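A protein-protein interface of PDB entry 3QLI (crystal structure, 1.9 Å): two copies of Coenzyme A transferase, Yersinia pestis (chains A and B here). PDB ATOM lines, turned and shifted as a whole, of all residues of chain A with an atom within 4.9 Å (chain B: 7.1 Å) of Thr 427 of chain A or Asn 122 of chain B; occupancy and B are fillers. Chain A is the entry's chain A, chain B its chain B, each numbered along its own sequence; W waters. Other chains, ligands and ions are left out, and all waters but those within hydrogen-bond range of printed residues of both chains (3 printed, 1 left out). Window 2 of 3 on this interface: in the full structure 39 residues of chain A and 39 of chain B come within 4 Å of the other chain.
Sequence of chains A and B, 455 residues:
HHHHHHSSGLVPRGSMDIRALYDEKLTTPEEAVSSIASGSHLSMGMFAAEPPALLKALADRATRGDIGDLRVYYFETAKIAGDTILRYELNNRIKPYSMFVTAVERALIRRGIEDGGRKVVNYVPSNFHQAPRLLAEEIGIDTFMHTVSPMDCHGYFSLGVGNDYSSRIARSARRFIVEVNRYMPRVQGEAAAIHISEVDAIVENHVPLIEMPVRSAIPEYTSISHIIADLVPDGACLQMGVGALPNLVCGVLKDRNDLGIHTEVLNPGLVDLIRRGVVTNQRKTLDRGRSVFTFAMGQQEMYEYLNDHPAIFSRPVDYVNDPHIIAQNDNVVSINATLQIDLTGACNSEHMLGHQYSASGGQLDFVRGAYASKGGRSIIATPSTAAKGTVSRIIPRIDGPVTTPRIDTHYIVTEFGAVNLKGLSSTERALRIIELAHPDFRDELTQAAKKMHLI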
ATOM      1  N   SER A 425      10.176 -11.243   5.247  1.00  0.00           N
ATOM      2  CA  SER A 425      10.583 -11.859   6.510  1.00  0.00           C
ATOM      3  C   SER A 425       9.826 -13.163   6.717  1.00  0.00           C
ATOM      4  O   SER A 425       8.854 -13.449   6.008  1.00  0.00           O
ATOM      5  CB  SER A 425      10.262 -10.928   7.681  1.00  0.00           C
ATOM      6  OG  SER A 425       8.855 -10.747   7.803  1.00  0.00           O
ATOM      7  N   SER A 426      10.249 -13.938   7.710  1.00  0.00           N
ATOM      8  CA  SER A 426       9.555 -15.165   8.069  1.00  0.00           C
ATOM      9  C   SER A 426       8.085 -14.903   8.411  1.00  0.00           C
ATOM     10  O   SER A 426       7.210 -15.704   8.087  1.00  0.00           O
ATOM     11  CB  SER A 426      10.243 -15.830   9.258  1.00  0.00           C
ATOM     12  OG  SER A 426      11.490 -16.369   8.859  1.00  0.00           O
ATOM     13  N   THR A 427       7.831 -13.787   9.081  1.00  0.00           N
ATOM     14  CA  THR A 427       6.467 -13.418   9.449  1.00  0.00           C
ATOM     15  C   THR A 427       5.642 -13.061   8.220  1.00  0.00           C
ATOM     16  O   THR A 427       4.509 -13.511   8.077  1.00  0.00           O
ATOM     17  CB  THR A 427       6.446 -12.224  10.427  1.00  0.00           C
ATOM     18  OG1 THR A 427       7.159 -12.574  11.617  1.00  0.00           O
ATOM     19  CG2 THR A 427       5.009 -11.843  10.783  1.00  0.00           C
ATOM     20  N   GLU A 428       6.202 -12.236   7.344  1.00  0.00           N
ATOM     21  CA  GLU A 428       5.491 -11.836   6.137  1.00  0.00           C
ATOM     22  C   GLU A 428       5.196 -13.053   5.251  1.00  0.00           C
ATOM     23  O   GLU A 428       4.118 -13.149   4.656  1.00  0.00           O
ATOM     24  CB  GLU A 428       6.283 -10.771   5.365  1.00  0.00           C
ATOM     25  CG  GLU A 428       6.390  -9.418   6.102  1.00  0.00           C
ATOM     26  CD  GLU A 428       7.431  -8.477   5.488  1.00  0.00           C
ATOM     27  OE1 GLU A 428       8.499  -8.955   5.061  1.00  0.00           O
ATOM     28  OE2 GLU A 428       7.185  -7.254   5.429  1.00  0.00           O
ATOM     29  N   ARG A 429       6.160 -13.968   5.150  1.00  0.00           N
ATOM     30  CA  ARG A 429       5.959 -15.200   4.392  1.00  0.00           C
ATOM     31  C   ARG A 429       4.824 -16.042   4.960  1.00  0.00           C
ATOM     32  O   ARG A 429       3.921 -16.452   4.227  1.00  0.00           O
ATOM     33  CB  ARG A 429       7.226 -16.053   4.365  1.00  0.00           C
ATOM     34  CG  ARG A 429       8.335 -15.469   3.546  1.00  0.00           C
ATOM     35  CD  ARG A 429       9.552 -16.388   3.523  1.00  0.00           C
ATOM     36  NE  ARG A 429      10.533 -15.896   2.563  1.00  0.00           N
ATOM     37  CZ  ARG A 429      11.186 -16.666   1.700  1.00  0.00           C
ATOM     38  NH1 ARG A 429      10.967 -17.970   1.677  1.00  0.00           N
ATOM     39  NH2 ARG A 429      12.053 -16.118   0.853  1.00  0.00           N
ATOM     40  N   ALA A 430       4.883 -16.327   6.259  1.00  0.00           N
ATOM     41  CA  ALA A 430       3.863 -17.173   6.875  1.00  0.00           C
ATOM     42  C   ALA A 430       2.472 -16.580   6.671  1.00  0.00           C
ATOM     43  O   ALA A 430       1.543 -17.283   6.283  1.00  0.00           O
ATOM     44  CB  ALA A 430       4.146 -17.386   8.374  1.00  0.00           C
ATOM     45  N   LEU A 431       2.336 -15.284   6.902  1.00  0.00           N
ATOM     46  CA  LEU A 431       1.025 -14.640   6.778  1.00  0.00           C
ATOM     47  C   LEU A 431       0.493 -14.705   5.346  1.00  0.00           C
ATOM     48  O   LEU A 431      -0.688 -14.973   5.124  1.00  0.00           O
ATOM     49  CB  LEU A 431       1.082 -13.186   7.255  1.00  0.00           C
ATOM     50  CG  LEU A 431       1.333 -12.954   8.754  1.00  0.00           C
ATOM     51  CD1 LEU A 431       1.583 -11.479   9.029  1.00  0.00           C
ATOM     52  CD2 LEU A 431       0.167 -13.464   9.612  1.00  0.00           C
ATOM     53  N   LEU A 454       7.004 -18.254  13.886  1.00  0.00           N
ATOM     54  CA  LEU A 454       7.120 -17.536  12.624  1.00  0.00           C
ATOM     55  C   LEU A 454       6.437 -16.177  12.731  1.00  0.00           C
ATOM     56  O   LEU A 454       6.901 -15.194  12.152  1.00  0.00           O
ATOM     57  CB  LEU A 454       6.529 -18.351  11.477  1.00  0.00           C
ATOM     58  CG  LEU A 454       7.250 -19.680  11.229  1.00  0.00           C
ATOM     59  CD1 LEU A 454       6.588 -20.466  10.100  1.00  0.00           C
ATOM     60  CD2 LEU A 454       8.735 -19.447  10.948  1.00  0.00           C
ATOM     61  N   ILE A 455       5.337 -16.115  13.480  1.00  0.00           N
ATOM     62  CA  ILE A 455       4.604 -14.862  13.617  1.00  0.00           C
ATOM     63  C   ILE A 455       4.437 -14.451  15.083  1.00  0.00           C
ATOM     64  O   ILE A 455       4.925 -15.135  15.982  1.00  0.00           O
ATOM     65  CB  ILE A 455       3.220 -14.921  12.911  1.00  0.00           C
ATOM     66  CG1 ILE A 455       2.255 -15.821  13.665  1.00  0.00           C
ATOM     67  CG2 ILE A 455       3.359 -15.437  11.484  1.00  0.00           C
ATOM     68  CD1 ILE A 455       0.987 -16.094  12.881  1.00  0.00           C
ATOM     69  N   VAL B  72      15.730  -2.584   9.973  1.00  0.00           N
ATOM     70  CA  VAL B  72      17.128  -2.637   9.586  1.00  0.00           C
ATOM     71  C   VAL B  72      17.438  -4.010   8.995  1.00  0.00           C
ATOM     72  O   VAL B  72      17.306  -5.031   9.662  1.00  0.00           O
ATOM     73  CB  VAL B  72      18.070  -2.345  10.760  1.00  0.00           C
ATOM     74  CG1 VAL B  72      19.542  -2.516  10.325  1.00  0.00           C
ATOM     75  CG2 VAL B  72      17.817  -0.917  11.305  1.00  0.00           C
ATOM     76  N   TYR B  73      17.845  -4.003   7.734  1.00  0.00           N
ATOM     77  CA  TYR B  73      18.173  -5.213   7.001  1.00  0.00           C
ATOM     78  C   TYR B  73      19.692  -5.272   6.872  1.00  0.00           C
ATOM     79  O   TYR B  73      20.311  -4.316   6.390  1.00  0.00           O
ATOM     80  CB  TYR B  73      17.569  -5.141   5.602  1.00  0.00           C
ATOM     81  CG  TYR B  73      16.059  -5.232   5.504  1.00  0.00           C
ATOM     82  CD1 TYR B  73      15.441  -6.434   5.160  1.00  0.00           C
ATOM     83  CD2 TYR B  73      15.248  -4.104   5.685  1.00  0.00           C
ATOM     84  CE1 TYR B  73      14.055  -6.527   5.019  1.00  0.00           C
ATOM     85  CE2 TYR B  73      13.856  -4.186   5.553  1.00  0.00           C
ATOM     86  CZ  TYR B  73      13.267  -5.406   5.222  1.00  0.00           C
ATOM     87  OH  TYR B  73      11.892  -5.512   5.089  1.00  0.00           O
ATOM     88  N   ASN B  91      14.068  -2.902  20.674  1.00  0.00           N
ATOM     89  CA  ASN B  91      13.488  -3.845  19.719  1.00  0.00           C
ATOM     90  C   ASN B  91      12.121  -3.436  19.165  1.00  0.00           C
ATOM     91  O   ASN B  91      11.742  -3.832  18.061  1.00  0.00           O
ATOM     92  CB  ASN B  91      13.409  -5.240  20.348  1.00  0.00           C
ATOM     93  CG  ASN B  91      13.145  -6.320  19.325  1.00  0.00           C
ATOM     94  OD1 ASN B  91      11.999  -6.691  19.080  1.00  0.00           O
ATOM     95  ND2 ASN B  91      14.215  -6.825  18.705  1.00  0.00           N
ATOM     96  N   LYS B  95      13.613  -2.436  14.397  1.00  0.00           N
ATOM     97  CA  LYS B  95      13.276  -3.844  14.222  1.00  0.00           C
ATOM     98  C   LYS B  95      14.319  -4.570  13.381  1.00  0.00           C
ATOM     99  O   LYS B  95      14.524  -4.215  12.227  1.00  0.00           O
ATOM    100  CB  LYS B  95      11.893  -3.938  13.575  1.00  0.00           C
ATOM    101  CG  LYS B  95      10.796  -3.360  14.484  1.00  0.00           C
ATOM    102  CD  LYS B  95       9.543  -2.986  13.716  1.00  0.00           C
ATOM    103  CE  LYS B  95       8.469  -2.465  14.675  1.00  0.00           C
ATOM    104  NZ  LYS B  95       7.268  -1.935  13.963  1.00  0.00           N
ATOM    105  N   PRO B  96      14.998  -5.568  13.964  1.00  0.00           N
ATOM    106  CA  PRO B  96      16.036  -6.279  13.210  1.00  0.00           C
ATOM    107  C   PRO B  96      15.435  -7.204  12.160  1.00  0.00           C
ATOM    108  O   PRO B  96      14.730  -8.163  12.494  1.00  0.00           O
ATOM    109  CB  PRO B  96      16.755  -7.106  14.281  1.00  0.00           C
ATOM    110  CG  PRO B  96      16.424  -6.409  15.582  1.00  0.00           C
ATOM    111  CD  PRO B  96      15.028  -5.919  15.393  1.00  0.00           C
ATOM    112  N   TYR B  97      15.715  -6.896  10.899  1.00  0.00           N
ATOM    113  CA  TYR B  97      15.364  -7.780   9.796  1.00  0.00           C
ATOM    114  C   TYR B  97      16.654  -8.467   9.373  1.00  0.00           C
ATOM    115  O   TYR B  97      17.233  -8.166   8.330  1.00  0.00           O
ATOM    116  CB  TYR B  97      14.688  -7.005   8.661  1.00  0.00           C
ATOM    117  CG  TYR B  97      13.193  -6.878   8.900  1.00  0.00           C
ATOM    118  CD1 TYR B  97      12.277  -7.569   8.115  1.00  0.00           C
ATOM    119  CD2 TYR B  97      12.705  -6.107   9.955  1.00  0.00           C
ATOM    120  CE1 TYR B  97      10.904  -7.480   8.362  1.00  0.00           C
ATOM    121  CE2 TYR B  97      11.344  -6.018  10.213  1.00  0.00           C
ATOM    122  CZ  TYR B  97      10.447  -6.705   9.413  1.00  0.00           C
ATOM    123  OH  TYR B  97       9.089  -6.604   9.667  1.00  0.00           O
ATOM    124  N   SER B  98      17.085  -9.388  10.227  1.00  0.00           N
ATOM    125  CA  SER B  98      18.407  -9.979  10.147  1.00  0.00           C
ATOM    126  C   SER B  98      18.465 -10.986   9.032  1.00  0.00           C
ATOM    127  O   SER B  98      17.573 -11.826   8.891  1.00  0.00           O
ATOM    128  CB  SER B  98      18.744 -10.657  11.466  1.00  0.00           C
ATOM    129  OG  SER B  98      18.322  -9.844  12.548  1.00  0.00           O
ATOM    130  N   MET B  99      19.521 -10.912   8.238  1.00  0.00           N
ATOM    131  CA  MET B  99      19.612 -11.797   7.087  1.00  0.00           C
ATOM    132  C   MET B  99      20.615 -12.941   7.284  1.00  0.00           C
ATOM    133  O   MET B  99      20.611 -13.908   6.523  1.00  0.00           O
ATOM    134  CB  MET B  99      19.823 -10.983   5.811  1.00  0.00           C
ATOM    135  CG  MET B  99      18.650 -10.027   5.592  1.00  0.00           C
ATOM    136  SD  MET B  99      18.810  -8.871   4.230  1.00  0.00           S
ATOM    137  CE  MET B  99      18.431  -9.943   2.838  1.00  0.00           C
ATOM    138  N   VAL B 101      21.629 -15.129  11.001  1.00  0.00           N
ATOM    139  CA  VAL B 101      21.407 -15.192  12.442  1.00  0.00           C
ATOM    140  C   VAL B 101      22.722 -15.567  13.127  1.00  0.00           C
ATOM    141  O   VAL B 101      23.199 -16.698  13.007  1.00  0.00           O
ATOM    142  CB  VAL B 101      20.294 -16.196  12.811  1.00  0.00           C
ATOM    143  CG1 VAL B 101      20.165 -16.330  14.306  1.00  0.00           C
ATOM    144  CG2 VAL B 101      18.959 -15.746  12.209  1.00  0.00           C
ATOM    145  N   ILE B 109      16.989 -13.647  20.412  1.00  0.00           N
ATOM    146  CA  ILE B 109      15.875 -14.563  20.207  1.00  0.00           C
ATOM    147  C   ILE B 109      15.532 -15.298  21.500  1.00  0.00           C
ATOM    148  O   ILE B 109      14.363 -15.429  21.862  1.00  0.00           O
ATOM    149  CB  ILE B 109      16.191 -15.583  19.084  1.00  0.00           C
ATOM    150  CG1 ILE B 109      16.160 -14.888  17.717  1.00  0.00           C
ATOM    151  CG2 ILE B 109      15.189 -16.738  19.109  1.00  0.00           C
ATOM    152  CD1 ILE B 109      16.792 -15.703  16.590  1.00  0.00           C
ATOM    153  N   LYS B 119       8.548 -12.617  19.533  1.00  0.00           N
ATOM    154  CA  LYS B 119       9.402 -12.601  18.354  1.00  0.00           C
ATOM    155  C   LYS B 119      10.061 -11.232  18.254  1.00  0.00           C
ATOM    156  O   LYS B 119       9.379 -10.214  18.163  1.00  0.00           O
ATOM    157  CB  LYS B 119       8.602 -12.883  17.082  1.00  0.00           C
ATOM    158  CG  LYS B 119       9.444 -12.757  15.815  1.00  0.00           C
ATOM    159  CD  LYS B 119       8.826 -13.477  14.628  1.00  0.00           C
ATOM    160  CE  LYS B 119       9.901 -13.788  13.593  1.00  0.00           C
ATOM    161  NZ  LYS B 119       9.448 -14.794  12.588  1.00  0.00           N
ATOM    162  N   VAL B 120      11.389 -11.214  18.260  1.00  0.00           N
ATOM    163  CA  VAL B 120      12.139  -9.965  18.342  1.00  0.00           C
ATOM    164  C   VAL B 120      13.160  -9.845  17.205  1.00  0.00           C
ATOM    165  O   VAL B 120      13.684  -8.765  16.927  1.00  0.00           O
ATOM    166  CB  VAL B 120      12.849  -9.843  19.716  1.00  0.00           C
ATOM    167  CG1 VAL B 120      11.821  -9.709  20.842  1.00  0.00           C
ATOM    168  CG2 VAL B 120      13.744 -11.051  19.967  1.00  0.00           C
ATOM    169  N   VAL B 121      13.445 -10.969  16.557  1.00  0.00           N
ATOM    170  CA  VAL B 121      14.275 -10.977  15.359  1.00  0.00           C
ATOM    171  C   VAL B 121      13.426 -11.441  14.174  1.00  0.00           C
ATOM    172  O   VAL B 121      12.826 -12.515  14.212  1.00  0.00           O
ATOM    173  CB  VAL B 121      15.498 -11.901  15.522  1.00  0.00           C
ATOM    174  CG1 VAL B 121      16.223 -12.083  14.185  1.00  0.00           C
ATOM    175  CG2 VAL B 121      16.445 -11.355  16.590  1.00  0.00           C
ATOM    176  N   ASN B 122      13.371 -10.623  13.129  1.00  0.00           N
ATOM    177  CA  ASN B 122      12.629 -10.971  11.920  1.00  0.00           C
ATOM    178  C   ASN B 122      13.540 -11.493  10.807  1.00  0.00           C
ATOM    179  O   ASN B 122      13.883 -10.755   9.884  1.00  0.00           O
ATOM    180  CB  ASN B 122      11.886  -9.748  11.391  1.00  0.00           C
ATOM    181  CG  ASN B 122      10.859  -9.230  12.363  1.00  0.00           C
ATOM    182  OD1 ASN B 122      11.171  -8.417  13.241  1.00  0.00           O
ATOM    183  ND2 ASN B 122       9.620  -9.698  12.219  1.00  0.00           N
ATOM    184  N   TYR B 123      13.910 -12.765  10.874  1.00  0.00           N
ATOM    185  CA  TYR B 123      14.778 -13.357   9.851  1.00  0.00           C
ATOM    186  C   TYR B 123      14.194 -13.225   8.455  1.00  0.00           C
ATOM    187  O   TYR B 123      13.014 -13.499   8.237  1.00  0.00           O
ATOM    188  CB  TYR B 123      15.029 -14.838  10.164  1.00  0.00           C
ATOM    189  CG  TYR B 123      15.822 -15.601   9.107  1.00  0.00           C
ATOM    190  CD1 TYR B 123      17.165 -15.314   8.860  1.00  0.00           C
ATOM    191  CD2 TYR B 123      15.237 -16.644   8.393  1.00  0.00           C
ATOM    192  CE1 TYR B 123      17.894 -16.036   7.897  1.00  0.00           C
ATOM    193  CE2 TYR B 123      15.942 -17.356   7.442  1.00  0.00           C
ATOM    194  CZ  TYR B 123      17.270 -17.057   7.195  1.00  0.00           C
ATOM    195  OH  TYR B 123      17.958 -17.794   6.246  1.00  0.00           O
ATOM    196  N   VAL B 124      15.028 -12.806   7.508  1.00  0.00           N
ATOM    197  CA  VAL B 124      14.632 -12.712   6.110  1.00  0.00           C
ATOM    198  C   VAL B 124      15.423 -13.761   5.320  1.00  0.00           C
ATOM    199  O   VAL B 124      16.631 -13.596   5.105  1.00  0.00           O
ATOM    200  CB  VAL B 124      14.947 -11.325   5.535  1.00  0.00           C
ATOM    201  CG1 VAL B 124      14.560 -11.256   4.061  1.00  0.00           C
ATOM    202  CG2 VAL B 124      14.227 -10.236   6.320  1.00  0.00           C
ATOM    203  N   PRO B 125      14.758 -14.855   4.919  1.00  0.00           N
ATOM    204  CA  PRO B 125      15.441 -15.901   4.150  1.00  0.00           C
ATOM    205  C   PRO B 125      15.942 -15.379   2.811  1.00  0.00           C
ATOM    206  O   PRO B 125      15.222 -14.668   2.107  1.00  0.00           O
ATOM    207  CB  PRO B 125      14.342 -16.945   3.917  1.00  0.00           C
ATOM    208  CG  PRO B 125      13.336 -16.689   5.003  1.00  0.00           C
ATOM    209  CD  PRO B 125      13.359 -15.210   5.213  1.00  0.00           C
HETATM  210  O   HOH W   1      10.801  -7.683   4.254  1.00  0.00           O
HETATM  211  O   HOH W   2       7.747  -8.948   9.358  1.00  0.00           O
HETATM  212  O   HOH W   3      12.767 -13.652   1.999  1.00  0.00           O
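Of chain B, only Lys 119 (3.3 Å) and Asn 122 (3.8 Å) come within 4 Å of Thr 427 of chain A. Asn 122 of chain B touches one residue of chain A. Of the printed residues of chain A, Tyr 123 of chain B touches Ser 425 (3.4 Å) and Ser 426 (2.8 Å). Of the printed residues of chain B, Ser 425 of chain A touches Tyr 97, Tyr 123 and Val 124. The nearest residue of chain A that does not touch Asn 122 of chain B is Ser 425 of chain A (4.2 Å). The nearest printed residue of chain B that does not touch Arg 429 of chain A is Val 124 of chain B (6.0 Å).
The backbone carbonyl oxygen of Tyr 123 of chain B lies within hydrogen-bond range of the backbone NH of Ser 426 of chain A (2.8 Å). NZ of Lys 119 of chain B is in hydrogen-bond range of OG1 of Thr 427 of chain A, 3.3 Å away. The side-chain amino group of Lys 119 of chain B sits at hydrogen-bond distance from the backbone carbonyl oxygen of Leu 454 of chain A (2.6 Å).
The side-chain hydroxyl (OG) of Ser 425 of chain A lies close to the backbone NH (N) of Thr 427 of chain A (3.5 Å). The backbone NH of Ser 425 of chain A lies within hydrogen-bond range of the side-chain carboxylate of Glu 428 of chain A, at 2.8 Å. The backbone carbonyl oxygen (O) of Val 72 of chain B lies within hydrogen-bond range of the backbone NH (N) of Tyr 97 of chain B (2.7 Å). O of Pro 96 of chain B is in hydrogen-bond range of N of Asn 122 of chain B (2.9 Å). The backbone carbonyl oxygen (O) of Asn 122 of chain B sits at hydrogen-bond distance from the backbone NH (N) of Ser 98 of chain B (3.5 Å). O of Ser 98 of chain B lies within hydrogen-bond range of N of Val 124 of chain B (3.1 Å).
No position is printed for both chains. Of the 9 pairs that touch across the chains among the printed residues, none has its exchanged pair printed and touching as well.
Water W1 bridges OH of Tyr 73 of chain B (2.6 Å) and OE1 of Glu 428 of chain A (2.8 Å). Water W2 bridges OG of Ser 425 of chain A (2.6 Å) and OH of Tyr 97 of chain B (2.7 Å). Water W3 lies within hydrogen-bond range of O of Pro 125 of chain B (2.7 Å) and NH2 of Arg 429 of chain A (2.8 Å).
Ser 425 of chain A touches Tyr 97 of chain B (CB to CE1, 3.6 Å). Ser 425 of chain A touches Tyr 123 of chain B (CA to O, 3.4 Å). Val 124 of chain B touches Ser 425 of chain A. CB of Ser 426 of chain A touches NZ of Lys 119 of chain B, 3.6 Å away. Thr 427 of chain A touches Asn 122 of chain B (OG1 to ND2, 3.8 Å). Pro 125 of chain B touches Arg 429 of chain A.
Of the 9 printed residues of chain A, 5 touch a printed residue of chain B. Among the printed residues, no Asp or Glu carboxylate lies within 4 Å of a Lys or Arg side-chain nitrogen of the other chain.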
